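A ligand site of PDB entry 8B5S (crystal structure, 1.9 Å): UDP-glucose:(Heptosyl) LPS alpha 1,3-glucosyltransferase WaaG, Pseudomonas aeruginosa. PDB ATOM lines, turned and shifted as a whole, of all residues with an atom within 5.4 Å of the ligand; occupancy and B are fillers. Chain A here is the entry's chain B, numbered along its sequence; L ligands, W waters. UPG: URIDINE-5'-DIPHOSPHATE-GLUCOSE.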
ATOM      1  N   PRO A  12     -10.590   0.710   5.250  1.00  0.00           N
ATOM      2  CA  PRO A  12      -9.774   1.633   4.456  1.00  0.00           C
ATOM      3  C   PRO A  12      -8.260   1.519   4.565  1.00  0.00           C
ATOM      4  O   PRO A  12      -7.554   1.949   3.654  1.00  0.00           O
ATOM      5  CB  PRO A  12     -10.254   3.020   4.936  1.00  0.00           C
ATOM      6  CG  PRO A  12     -10.790   2.781   6.329  1.00  0.00           C
ATOM      7  CD  PRO A  12     -11.353   1.379   6.321  1.00  0.00           C
ATOM      8  N   PHE A  13      -7.738   0.910   5.648  1.00  0.00           N
ATOM      9  CA  PHE A  13      -6.331   1.033   5.988  1.00  0.00           C
ATOM     10  C   PHE A  13      -5.561  -0.239   5.669  1.00  0.00           C
ATOM     11  O   PHE A  13      -4.731  -0.689   6.457  1.00  0.00           O
ATOM     12  CB  PHE A  13      -6.175   1.394   7.471  1.00  0.00           C
ATOM     13  CG  PHE A  13      -7.017   2.572   7.915  1.00  0.00           C
ATOM     14  CD1 PHE A  13      -7.219   3.653   7.077  1.00  0.00           C
ATOM     15  CD2 PHE A  13      -7.569   2.598   9.186  1.00  0.00           C
ATOM     16  CE1 PHE A  13      -7.988   4.725   7.483  1.00  0.00           C
ATOM     17  CE2 PHE A  13      -8.339   3.679   9.596  1.00  0.00           C
ATOM     18  CZ  PHE A  13      -8.540   4.741   8.751  1.00  0.00           C
ATOM     19  N   GLY A  14      -5.822  -0.804   4.491  1.00  0.00           N
ATOM     20  CA  GLY A  14      -5.093  -1.968   3.999  1.00  0.00           C
ATOM     21  C   GLY A  14      -4.878  -1.842   2.494  1.00  0.00           C
ATOM     22  O   GLY A  14      -5.703  -1.245   1.805  1.00  0.00           O
ATOM     23  N   GLY A  15      -3.759  -2.415   2.024  1.00  0.00           N
ATOM     24  CA  GLY A  15      -3.376  -2.357   0.611  1.00  0.00           C
ATOM     25  C   GLY A  15      -4.337  -3.130  -0.287  1.00  0.00           C
ATOM     26  O   GLY A  15      -4.739  -2.636  -1.337  1.00  0.00           O
ATOM     27  N   LEU A  16      -4.697  -4.348   0.125  1.00  0.00           N
ATOM     28  CA  LEU A  16      -5.637  -5.187  -0.610  1.00  0.00           C
ATOM     29  C   LEU A  16      -6.950  -4.441  -0.782  1.00  0.00           C
ATOM     30  O   LEU A  16      -7.521  -4.392  -1.866  1.00  0.00           O
ATOM     31  CB  LEU A  16      -5.809  -6.498   0.160  1.00  0.00           C
ATOM     32  CG  LEU A  16      -6.707  -7.564  -0.489  1.00  0.00           C
ATOM     33  CD1 LEU A  16      -6.474  -8.925   0.154  1.00  0.00           C
ATOM     34  CD2 LEU A  16      -8.181  -7.187  -0.395  1.00  0.00           C
ATOM     35  N   ARG A  18      -7.577  -1.130  -0.427  1.00  0.00           N
ATOM     36  CA  ARG A  18      -7.455   0.082  -1.233  1.00  0.00           C
ATOM     37  C   ARG A  18      -7.337  -0.260  -2.713  1.00  0.00           C
ATOM     38  O   ARG A  18      -7.844   0.487  -3.547  1.00  0.00           O
ATOM     39  CB  ARG A  18      -6.256   0.915  -0.766  1.00  0.00           C
ATOM     40  CG  ARG A  18      -6.533   1.719   0.499  1.00  0.00           C
ATOM     41  CD  ARG A  18      -5.305   2.419   1.052  1.00  0.00           C
ATOM     42  NE  ARG A  18      -4.680   3.315   0.093  1.00  0.00           N
ATOM     43  CZ  ARG A  18      -5.164   4.488  -0.276  1.00  0.00           C
ATOM     44  NH1 ARG A  18      -6.232   4.995   0.309  1.00  0.00           N
ATOM     45  NH2 ARG A  18      -4.551   5.181  -1.237  1.00  0.00           N
ATOM     46  N   ASP A  19      -6.674  -1.370  -3.045  1.00  0.00           N
ATOM     47  CA  ASP A  19      -6.511  -1.794  -4.428  1.00  0.00           C
ATOM     48  C   ASP A  19      -7.858  -2.210  -5.006  1.00  0.00           C
ATOM     49  O   ASP A  19      -8.201  -1.814  -6.124  1.00  0.00           O
ATOM     50  CB  ASP A  19      -5.489  -2.935  -4.554  1.00  0.00           C
ATOM     51  CG  ASP A  19      -4.033  -2.519  -4.367  1.00  0.00           C
ATOM     52  OD1 ASP A  19      -3.770  -1.313  -4.195  1.00  0.00           O
ATOM     53  OD2 ASP A  19      -3.170  -3.419  -4.411  1.00  0.00           O
ATOM     54  N   ALA A  98      -3.969 -11.042  -7.205  1.00  0.00           N
ATOM     55  CA  ALA A  98      -3.041 -11.752  -6.343  1.00  0.00           C
ATOM     56  C   ALA A  98      -2.378 -10.795  -5.367  1.00  0.00           C
ATOM     57  O   ALA A  98      -1.204 -10.451  -5.487  1.00  0.00           O
ATOM     58  CB  ALA A  98      -2.015 -12.484  -7.182  1.00  0.00           C
ATOM     59  N   ALA A  99      -3.158 -10.369  -4.368  1.00  0.00           N
ATOM     60  CA  ALA A  99      -2.652  -9.538  -3.295  1.00  0.00           C
ATOM     61  C   ALA A  99      -1.668 -10.347  -2.438  1.00  0.00           C
ATOM     62  O   ALA A  99      -0.625  -9.835  -2.044  1.00  0.00           O
ATOM     63  CB  ALA A  99      -3.808  -8.992  -2.484  1.00  0.00           C
ATOM     64  N   ASP A 100      -1.971 -11.628  -2.190  1.00  0.00           N
ATOM     65  CA  ASP A 100      -1.203 -12.451  -1.270  1.00  0.00           C
ATOM     66  C   ASP A 100      -0.079 -13.180  -1.993  1.00  0.00           C
ATOM     67  O   ASP A 100      -0.102 -13.328  -3.221  1.00  0.00           O
ATOM     68  CB  ASP A 100      -2.111 -13.463  -0.558  1.00  0.00           C
ATOM     69  CG  ASP A 100      -3.063 -12.832   0.441  1.00  0.00           C
ATOM     70  OD1 ASP A 100      -2.569 -12.112   1.341  1.00  0.00           O
ATOM     71  OD2 ASP A 100      -4.286 -13.078   0.328  1.00  0.00           O
ATOM     72  N   ILE A 143       0.871  -8.620  -9.078  1.00  0.00           N
ATOM     73  CA  ILE A 143       1.528  -7.362  -8.749  1.00  0.00           C
ATOM     74  C   ILE A 143       2.976  -7.625  -8.329  1.00  0.00           C
ATOM     75  O   ILE A 143       3.731  -6.677  -8.118  1.00  0.00           O
ATOM     76  CB  ILE A 143       0.719  -6.616  -7.669  1.00  0.00           C
ATOM     77  CG1 ILE A 143       0.553  -7.419  -6.374  1.00  0.00           C
ATOM     78  CG2 ILE A 143      -0.635  -6.198  -8.231  1.00  0.00           C
ATOM     79  CD1 ILE A 143      -0.157  -6.678  -5.278  1.00  0.00           C
ATOM     80  N   ARG A 173      -1.496  10.816  -2.357  1.00  0.00           N
ATOM     81  CA  ARG A 173      -0.206  10.514  -1.753  1.00  0.00           C
ATOM     82  C   ARG A 173       0.901  11.384  -2.362  1.00  0.00           C
ATOM     83  O   ARG A 173       1.959  11.514  -1.760  1.00  0.00           O
ATOM     84  CB  ARG A 173       0.150   9.038  -1.899  1.00  0.00           C
ATOM     85  CG  ARG A 173      -0.217   8.175  -0.707  1.00  0.00           C
ATOM     86  CD  ARG A 173      -1.699   8.093  -0.428  1.00  0.00           C
ATOM     87  NE  ARG A 173      -1.989   7.112   0.605  1.00  0.00           N
ATOM     88  CZ  ARG A 173      -3.080   7.108   1.364  1.00  0.00           C
ATOM     89  NH1 ARG A 173      -3.984   8.060   1.247  1.00  0.00           N
ATOM     90  NH2 ARG A 173      -3.259   6.139   2.249  1.00  0.00           N
ATOM     91  N   ILE A 202       4.899   2.380   8.702  1.00  0.00           N
ATOM     92  CA  ILE A 202       3.483   2.433   8.372  1.00  0.00           C
ATOM     93  C   ILE A 202       3.029   1.088   7.810  1.00  0.00           C
ATOM     94  O   ILE A 202       3.652   0.549   6.903  1.00  0.00           O
ATOM     95  CB  ILE A 202       3.190   3.601   7.409  1.00  0.00           C
ATOM     96  CG1 ILE A 202       3.572   4.952   8.024  1.00  0.00           C
ATOM     97  CG2 ILE A 202       1.725   3.588   6.980  1.00  0.00           C
ATOM     98  CD1 ILE A 202       3.439   6.124   7.070  1.00  0.00           C
ATOM     99  N   GLY A 203       1.935   0.574   8.380  1.00  0.00           N
ATOM    100  CA  GLY A 203       1.313  -0.654   7.917  1.00  0.00           C
ATOM    101  C   GLY A 203       1.017  -1.606   9.079  1.00  0.00           C
ATOM    102  O   GLY A 203       1.880  -1.856   9.915  1.00  0.00           O
ATOM    103  N   SER A 204      -0.207  -2.149   9.083  1.00  0.00           N
ATOM    104  CA  SER A 204      -0.594  -3.170  10.050  1.00  0.00           C
ATOM    105  C   SER A 204       0.211  -4.433   9.807  1.00  0.00           C
ATOM    106  O   SER A 204       0.505  -4.780   8.671  1.00  0.00           O
ATOM    107  CB  SER A 204      -2.079  -3.439   9.978  1.00  0.00           C
ATOM    108  OG  SER A 204      -2.816  -2.272  10.307  1.00  0.00           O
ATOM    109  N   LYS A 209       6.559  -6.680   9.361  1.00  0.00           N
ATOM    110  CA  LYS A 209       7.097  -5.481   8.725  1.00  0.00           C
ATOM    111  C   LYS A 209       8.325  -4.965   9.470  1.00  0.00           C
ATOM    112  O   LYS A 209       8.929  -3.973   9.051  1.00  0.00           O
ATOM    113  CB  LYS A 209       5.979  -4.439   8.590  1.00  0.00           C
ATOM    114  CG  LYS A 209       4.899  -4.817   7.590  1.00  0.00           C
ATOM    115  CD  LYS A 209       3.709  -3.892   7.582  1.00  0.00           C
ATOM    116  CE  LYS A 209       2.623  -4.314   6.617  1.00  0.00           C
ATOM    117  NZ  LYS A 209       3.013  -4.113   5.195  1.00  0.00           N
ATOM    118  N   ILE A 234       2.312   3.102  12.690  1.00  0.00           N
ATOM    119  CA  ILE A 234       0.890   3.261  12.421  1.00  0.00           C
ATOM    120  C   ILE A 234       0.329   1.952  11.874  1.00  0.00           C
ATOM    121  O   ILE A 234       0.716   1.497  10.802  1.00  0.00           O
ATOM    122  CB  ILE A 234       0.639   4.437  11.446  1.00  0.00           C
ATOM    123  CG1 ILE A 234       1.332   5.720  11.899  1.00  0.00           C
ATOM    124  CG2 ILE A 234      -0.863   4.655  11.259  1.00  0.00           C
ATOM    125  CD1 ILE A 234       1.155   6.889  10.969  1.00  0.00           C
ATOM    126  N   GLY A 235      -0.597   1.366  12.643  1.00  0.00           N
ATOM    127  CA  GLY A 235      -1.189   0.079  12.294  1.00  0.00           C
ATOM    128  C   GLY A 235      -2.237  -0.337  13.330  1.00  0.00           C
ATOM    129  O   GLY A 235      -2.277   0.200  14.432  1.00  0.00           O
ATOM    130  N   LYS A 259      -2.975   3.798  16.103  1.00  0.00           N
ATOM    131  CA  LYS A 259      -3.929   2.987  15.376  1.00  0.00           C
ATOM    132  C   LYS A 259      -4.038   3.480  13.937  1.00  0.00           C
ATOM    133  O   LYS A 259      -3.611   4.597  13.619  1.00  0.00           O
ATOM    134  CB  LYS A 259      -5.287   3.026  16.081  1.00  0.00           C
ATOM    135  CG  LYS A 259      -5.346   2.259  17.398  1.00  0.00           C
ATOM    136  CD  LYS A 259      -5.259   0.753  17.223  1.00  0.00           C
ATOM    137  CE  LYS A 259      -5.437  -0.009  18.521  1.00  0.00           C
ATOM    138  NZ  LYS A 259      -5.226  -1.462  18.324  1.00  0.00           N
ATOM    139  N   GLY A 260      -4.614   2.644  13.065  1.00  0.00           N
ATOM    140  CA  GLY A 260      -4.818   2.992  11.673  1.00  0.00           C
ATOM    141  C   GLY A 260      -5.536   4.331  11.517  1.00  0.00           C
ATOM    142  O   GLY A 260      -6.353   4.701  12.358  1.00  0.00           O
ATOM    143  N   ARG A 261      -5.236   5.053  10.433  1.00  0.00           N
ATOM    144  CA  ARG A 261      -5.828   6.364  10.214  1.00  0.00           C
ATOM    145  C   ARG A 261      -5.753   6.761   8.741  1.00  0.00           C
ATOM    146  O   ARG A 261      -4.975   6.197   7.983  1.00  0.00           O
ATOM    147  CB  ARG A 261      -5.155   7.398  11.124  1.00  0.00           C
ATOM    148  CG  ARG A 261      -3.636   7.302  11.153  1.00  0.00           C
ATOM    149  CD  ARG A 261      -3.124   8.077  12.359  1.00  0.00           C
ATOM    150  NE  ARG A 261      -3.545   9.471  12.289  1.00  0.00           N
ATOM    151  CZ  ARG A 261      -3.646  10.275  13.338  1.00  0.00           C
ATOM    152  NH1 ARG A 261      -3.494   9.802  14.554  1.00  0.00           N
ATOM    153  NH2 ARG A 261      -3.928  11.555  13.154  1.00  0.00           N
ATOM    154  N   SER A 262      -6.559   7.767   8.380  1.00  0.00           N
ATOM    155  CA  SER A 262      -6.761   8.118   6.978  1.00  0.00           C
ATOM    156  C   SER A 262      -5.760   9.173   6.506  1.00  0.00           C
ATOM    157  O   SER A 262      -5.554   9.311   5.296  1.00  0.00           O
ATOM    158  CB  SER A 262      -8.186   8.590   6.759  1.00  0.00           C
ATOM    159  OG  SER A 262      -8.516   9.669   7.618  1.00  0.00           O
ATOM    160  N   ILE A 264      -2.561   9.554   6.255  1.00  0.00           N
ATOM    161  CA  ILE A 264      -1.195   9.072   6.059  1.00  0.00           C
ATOM    162  C   ILE A 264      -0.357  10.125   5.328  1.00  0.00           C
ATOM    163  O   ILE A 264       0.795  10.338   5.697  1.00  0.00           O
ATOM    164  CB  ILE A 264      -1.197   7.719   5.329  1.00  0.00           C
ATOM    165  CG1 ILE A 264      -1.814   6.613   6.190  1.00  0.00           C
ATOM    166  CG2 ILE A 264       0.193   7.342   4.841  1.00  0.00           C
ATOM    167  CD1 ILE A 264      -1.100   6.369   7.510  1.00  0.00           C
ATOM    168  N   HIS A 276      11.344   0.543   6.877  1.00  0.00           N
ATOM    169  CA  HIS A 276      10.535  -0.605   6.518  1.00  0.00           C
ATOM    170  C   HIS A 276      11.435  -1.821   6.352  1.00  0.00           C
ATOM    171  O   HIS A 276      11.617  -2.316   5.239  1.00  0.00           O
ATOM    172  CB  HIS A 276       9.736  -0.302   5.248  1.00  0.00           C
ATOM    173  CG  HIS A 276       8.545  -1.188   5.055  1.00  0.00           C
ATOM    174  ND1 HIS A 276       7.319  -0.903   5.615  1.00  0.00           N
ATOM    175  CD2 HIS A 276       8.378  -2.308   4.338  1.00  0.00           C
ATOM    176  CE1 HIS A 276       6.450  -1.844   5.256  1.00  0.00           C
ATOM    177  NE2 HIS A 276       7.078  -2.709   4.489  1.00  0.00           N
ATOM    178  N   GLU A 281       7.541  -9.046   2.320  1.00  0.00           N
ATOM    179  CA  GLU A 281       6.602  -8.041   1.858  1.00  0.00           C
ATOM    180  C   GLU A 281       6.413  -8.248   0.350  1.00  0.00           C
ATOM    181  O   GLU A 281       7.365  -8.079  -0.407  1.00  0.00           O
ATOM    182  CB  GLU A 281       7.135  -6.630   2.167  1.00  0.00           C
ATOM    183  CG  GLU A 281       6.144  -5.514   1.889  1.00  0.00           C
ATOM    184  CD  GLU A 281       5.042  -5.372   2.928  1.00  0.00           C
ATOM    185  OE1 GLU A 281       3.883  -5.700   2.612  1.00  0.00           O
ATOM    186  OE2 GLU A 281       5.348  -4.935   4.056  1.00  0.00           O
ATOM    187  N   ASN A 282       5.192  -8.627  -0.050  1.00  0.00           N
ATOM    188  CA  ASN A 282       4.903  -8.974  -1.434  1.00  0.00           C
ATOM    189  C   ASN A 282       5.217  -7.783  -2.330  1.00  0.00           C
ATOM    190  O   ASN A 282       5.872  -7.941  -3.372  1.00  0.00           O
ATOM    191  CB  ASN A 282       3.462  -9.479  -1.575  1.00  0.00           C
ATOM    192  CG  ASN A 282       3.128 -10.037  -2.949  1.00  0.00           C
ATOM    193  OD1 ASN A 282       3.838 -10.897  -3.461  1.00  0.00           O
ATOM    194  ND2 ASN A 282       2.053  -9.554  -3.543  1.00  0.00           N
ATOM    195  N   THR A 283       4.772  -6.585  -1.936  1.00  0.00           N
ATOM    196  CA  THR A 283       5.095  -5.375  -2.672  1.00  0.00           C
ATOM    197  C   THR A 283       5.572  -4.284  -1.713  1.00  0.00           C
ATOM    198  O   THR A 283       6.773  -4.042  -1.595  1.00  0.00           O
ATOM    199  CB  THR A 283       3.924  -4.923  -3.544  1.00  0.00           C
ATOM    200  OG1 THR A 283       2.763  -4.764  -2.726  1.00  0.00           O
ATOM    201  CG2 THR A 283       3.630  -5.892  -4.673  1.00  0.00           C
ATOM    202  N   GLY A 284       4.621  -3.628  -1.029  1.00  0.00           N
ATOM    203  CA  GLY A 284       4.930  -2.547  -0.094  1.00  0.00           C
ATOM    204  C   GLY A 284       4.581  -1.180  -0.669  1.00  0.00           C
ATOM    205  O   GLY A 284       5.458  -0.387  -0.981  1.00  0.00           O
ATOM    206  N   THR A 285       3.268  -0.933  -0.789  1.00  0.00           N
ATOM    207  CA  THR A 285       2.729   0.319  -1.311  1.00  0.00           C
ATOM    208  C   THR A 285       3.308   1.534  -0.580  1.00  0.00           C
ATOM    209  O   THR A 285       3.565   2.549  -1.206  1.00  0.00           O
ATOM    210  CB  THR A 285       1.199   0.303  -1.266  1.00  0.00           C
ATOM    211  OG1 THR A 285       0.791  -0.671  -2.234  1.00  0.00           O
ATOM    212  CG2 THR A 285       0.565   1.633  -1.583  1.00  0.00           C
ATOM    213  N   VAL A 286       3.495   1.421   0.745  1.00  0.00           N
ATOM    214  CA  VAL A 286       3.961   2.557   1.545  1.00  0.00           C
ATOM    215  C   VAL A 286       5.351   2.999   1.090  1.00  0.00           C
ATOM    216  O   VAL A 286       5.699   4.173   1.255  1.00  0.00           O
ATOM    217  CB  VAL A 286       3.946   2.260   3.056  1.00  0.00           C
ATOM    218  CG1 VAL A 286       2.537   1.986   3.570  1.00  0.00           C
ATOM    219  CG2 VAL A 286       4.905   1.133   3.444  1.00  0.00           C
ATOM    220  N   LEU A 287       6.140   2.078   0.505  1.00  0.00           N
ATOM    221  CA  LEU A 287       7.463   2.414  -0.002  1.00  0.00           C
ATOM    222  C   LEU A 287       7.342   3.475  -1.092  1.00  0.00           C
ATOM    223  O   LEU A 287       8.100   4.446  -1.100  1.00  0.00           O
ATOM    224  CB  LEU A 287       8.172   1.164  -0.529  1.00  0.00           C
ATOM    225  CG  LEU A 287       8.363   0.023   0.479  1.00  0.00           C
ATOM    226  CD1 LEU A 287       8.971  -1.203  -0.209  1.00  0.00           C
ATOM    227  CD2 LEU A 287       9.224   0.456   1.645  1.00  0.00           C
ATOM    228  N   GLU A 289       4.546   5.329  -1.681  1.00  0.00           N
ATOM    229  CA  GLU A 289       3.859   6.490  -1.139  1.00  0.00           C
ATOM    230  C   GLU A 289       4.874   7.462  -0.547  1.00  0.00           C
ATOM    231  O   GLU A 289       4.757   8.673  -0.725  1.00  0.00           O
ATOM    232  CB  GLU A 289       2.809   6.061  -0.096  1.00  0.00           C
ATOM    233  CG  GLU A 289       1.703   5.186  -0.659  1.00  0.00           C
ATOM    234  CD  GLU A 289       0.612   4.804   0.328  1.00  0.00           C
ATOM    235  OE1 GLU A 289       0.943   4.605   1.518  1.00  0.00           O
ATOM    236  OE2 GLU A 289      -0.562   4.687  -0.106  1.00  0.00           O
HETATM  237  N1  UPG L   1      -2.725   2.666   5.184  1.00  0.00           N
HETATM  238  C2  UPG L   1      -3.605   3.667   5.544  1.00  0.00           C
HETATM  239  N3  UPG L   1      -3.692   3.886   6.898  1.00  0.00           N
HETATM  240  C4  UPG L   1      -3.019   3.225   7.903  1.00  0.00           C
HETATM  241  C5  UPG L   1      -2.130   2.195   7.448  1.00  0.00           C
HETATM  242  C6  UPG L   1      -2.008   1.958   6.126  1.00  0.00           C
HETATM  243  O2  UPG L   1      -4.256   4.312   4.742  1.00  0.00           O
HETATM  244  O4  UPG L   1      -3.207   3.538   9.078  1.00  0.00           O
HETATM  245  C1C UPG L   1      -2.558   2.389   3.748  1.00  0.00           C
HETATM  246  C2C UPG L   1      -1.164   2.779   3.231  1.00  0.00           C
HETATM  247  O2C UPG L   1      -1.096   4.173   3.014  1.00  0.00           O
HETATM  248  C3C UPG L   1      -1.128   1.929   1.959  1.00  0.00           C
HETATM  249  C4C UPG L   1      -1.782   0.614   2.432  1.00  0.00           C
HETATM  250  O4C UPG L   1      -2.676   1.001   3.503  1.00  0.00           O
HETATM  251  O3C UPG L   1      -1.874   2.561   0.918  1.00  0.00           O
HETATM  252  C5C UPG L   1      -0.836  -0.455   2.925  1.00  0.00           C
HETATM  253  O5C UPG L   1      -0.281  -1.142   1.778  1.00  0.00           O
HETATM  254  PA  UPG L   1       1.142  -1.889   1.808  1.00  0.00           P
HETATM  255  O1A UPG L   1       2.224  -0.962   2.277  1.00  0.00           O
HETATM  256  O2A UPG L   1       1.351  -2.604   0.509  1.00  0.00           O
HETATM  257  O3A UPG L   1       0.883  -2.971   2.960  1.00  0.00           O
HETATM  258  PB  UPG L   1      -0.020  -4.300   3.057  1.00  0.00           P
HETATM  259  O1B UPG L   1       0.440  -5.047   4.273  1.00  0.00           O
HETATM  260  O2B UPG L   1      -1.452  -3.891   2.987  1.00  0.00           O
HETATM  261  O3B UPG L   1       0.423  -5.117   1.732  1.00  0.00           O
HETATM  262  C1' UPG L   1       0.959  -6.424   1.769  1.00  0.00           C
HETATM  263  C2' UPG L   1       1.711  -6.706   0.472  1.00  0.00           C
HETATM  264  C3' UPG L   1       0.746  -6.609  -0.689  1.00  0.00           C
HETATM  265  C4' UPG L   1      -0.408  -7.564  -0.489  1.00  0.00           C
HETATM  266  C5' UPG L   1      -1.070  -7.419   0.893  1.00  0.00           C
HETATM  267  C6' UPG L   1      -1.983  -8.578   1.203  1.00  0.00           C
HETATM  268  O2' UPG L   1       2.819  -5.836   0.318  1.00  0.00           O
HETATM  269  O3' UPG L   1       1.394  -6.903  -1.923  1.00  0.00           O
HETATM  270  O4' UPG L   1      -1.392  -7.313  -1.488  1.00  0.00           O
HETATM  271  O5' UPG L   1      -0.068  -7.389   1.945  1.00  0.00           O
HETATM  272  O6' UPG L   1      -2.925  -8.239   2.215  1.00  0.00           O
HETATM  273  O   HOH W   1      -3.382  -5.624   2.483  1.00  0.00           O
HETATM  274  O   HOH W   2      -5.970   6.813   3.869  1.00  0.00           O
HETATM  275  O   HOH W   3      -1.939  -1.453   6.789  1.00  0.00           O
HETATM  276  O   HOH W   4       2.900  -1.382   4.996  1.00  0.00           O
HETATM  277  O   HOH W   5       0.461  -7.450   5.117  1.00  0.00           O
HETATM  278  O   HOH W   6      -0.693  -3.015  -1.430  1.00  0.00           O
HETATM  279  O   HOH W   7      -1.022  -4.062   6.468  1.00  0.00           O
HETATM  280  O   HOH W   8      -2.281  -4.934  -2.329  1.00  0.00           O
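The backbone NH of Arg 261 lies within hydrogen-bond range of an oxygen (O4) of the ligand (2.9 Å). O of Arg 261 sits at hydrogen-bond distance from N3 of the ligand (2.9 Å). The side-chain hydroxyl (OG1) of Thr 285 sits at hydrogen-bond distance from an oxygen (O2A) of the ligand. O2A of the ligand lies within hydrogen-bond range of N of Thr 285 (2.9 Å). NH2 of Arg 173 sits at hydrogen-bond distance from O2C of the ligand (3.0 Å). The backbone NH of Gly 284 sits at hydrogen-bond distance from an oxygen (O2') of the ligand, at 3.2 Å. The side-chain carboxylate (OE1) of Glu 281 lies within hydrogen-bond range of an oxygen (O2') of the ligand, at 2.5 Å. The side-chain amide nitrogen (ND2) of Asn 282 is in hydrogen-bond range of an oxygen (O3') of the ligand. O3C of the ligand lies within hydrogen-bond range of NE of Arg 18, at 3.0 Å. The side-chain hydroxyl (OG1) of Thr 283 sits at hydrogen-bond distance from an oxygen (O3') of the ligand. N of Gly 15 sits at hydrogen-bond distance from O2B of the ligand (2.9 Å). O of Ala 99 sits at hydrogen-bond distance from O4' of the ligand (2.7 Å). OE1 of Glu 289 is in hydrogen-bond range of O2C of the ligand. O2' of the ligand is in hydrogen-bond range of N of Thr 283, at 3.1 Å. NZ of Lys 209 lies within salt-bridge range of O1B of the ligand, 2.9 Å away. An oxygen (O1A) of the ligand lies within hydrogen-bond range of the backbone NH of Val 286.
Water W8 lies within hydrogen-bond range of an oxygen (O4') of the ligand (2.7 Å), the side-chain carboxylate (OD2) of Asp 19 (2.7 Å) and the backbone NH (N) of Leu 16 (3.5 Å). Water W7 bridges O of Ser 204 and O1B of the ligand. Water W4 lies within hydrogen-bond range of NZ of Lys 209 (2.7 Å), O of Ile 202 (2.8 Å) and O1A of the ligand (2.8 Å). Water W6 lies within hydrogen-bond range of an oxygen (O2A) of the ligand (2.8 Å) and the side-chain hydroxyl of Thr 285 (2.9 Å). Water W2 lies within hydrogen-bond range of the backbone carbonyl oxygen (O) of Ser 262 (2.9 Å), an oxygen (O2) of the ligand (3.2 Å) and the guanidinium group (NH2) of Arg 173 (3.2 Å). Water W3 bridges the backbone carbonyl oxygen (O) of Phe 13 and the backbone NH (N) of Ser 204.
O of Ile 234 lies within hydrogen-bond range of N of Gly 203, 2.9 Å away. The side-chain carboxylate of Glu 289 is in salt-bridge range of the guanidinium group of Arg 173, 2.9 Å away. O of Ala 99 sits at hydrogen-bond distance from ND2 of Asn 282 (3.1 Å). The side-chain carboxylate of Glu 281 is in salt-bridge range of the side-chain amino group of Lys 209 (2.7 Å). The side-chain carboxylate of Glu 281 is in hydrogen-bond range of a ring nitrogen (NE2) of His 276 (2.9 Å).
Phe 13 touches the ligand. C of Gly 14 touches O4C of the ligand (3.7 Å). Leu 16 touches the ligand (CB to O6', 3.9 Å). Asp 100 touches the ligand. CD1 of Ile 143 touches O3' of the ligand (3.7 Å). CG2 of Ile 234 touches O4 of the ligand, at 3.4 Å. Gly 260 touches the ligand. CG1 of Ile 264 touches N3 of the ligand, 3.4 Å away. 21 residues have an atom within 4 Å of the ligand: Phe 13, Gly 14, Gly 15, Leu 16, Arg 18, Ala 99, Asp 100, Ile 143, Arg 173, Lys 209, Ile 234, Gly 260, Arg 261, Ile 264, Glu 281, Asn 282, Thr 283, Gly 284, Thr 285, Val 286 and Glu 289.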
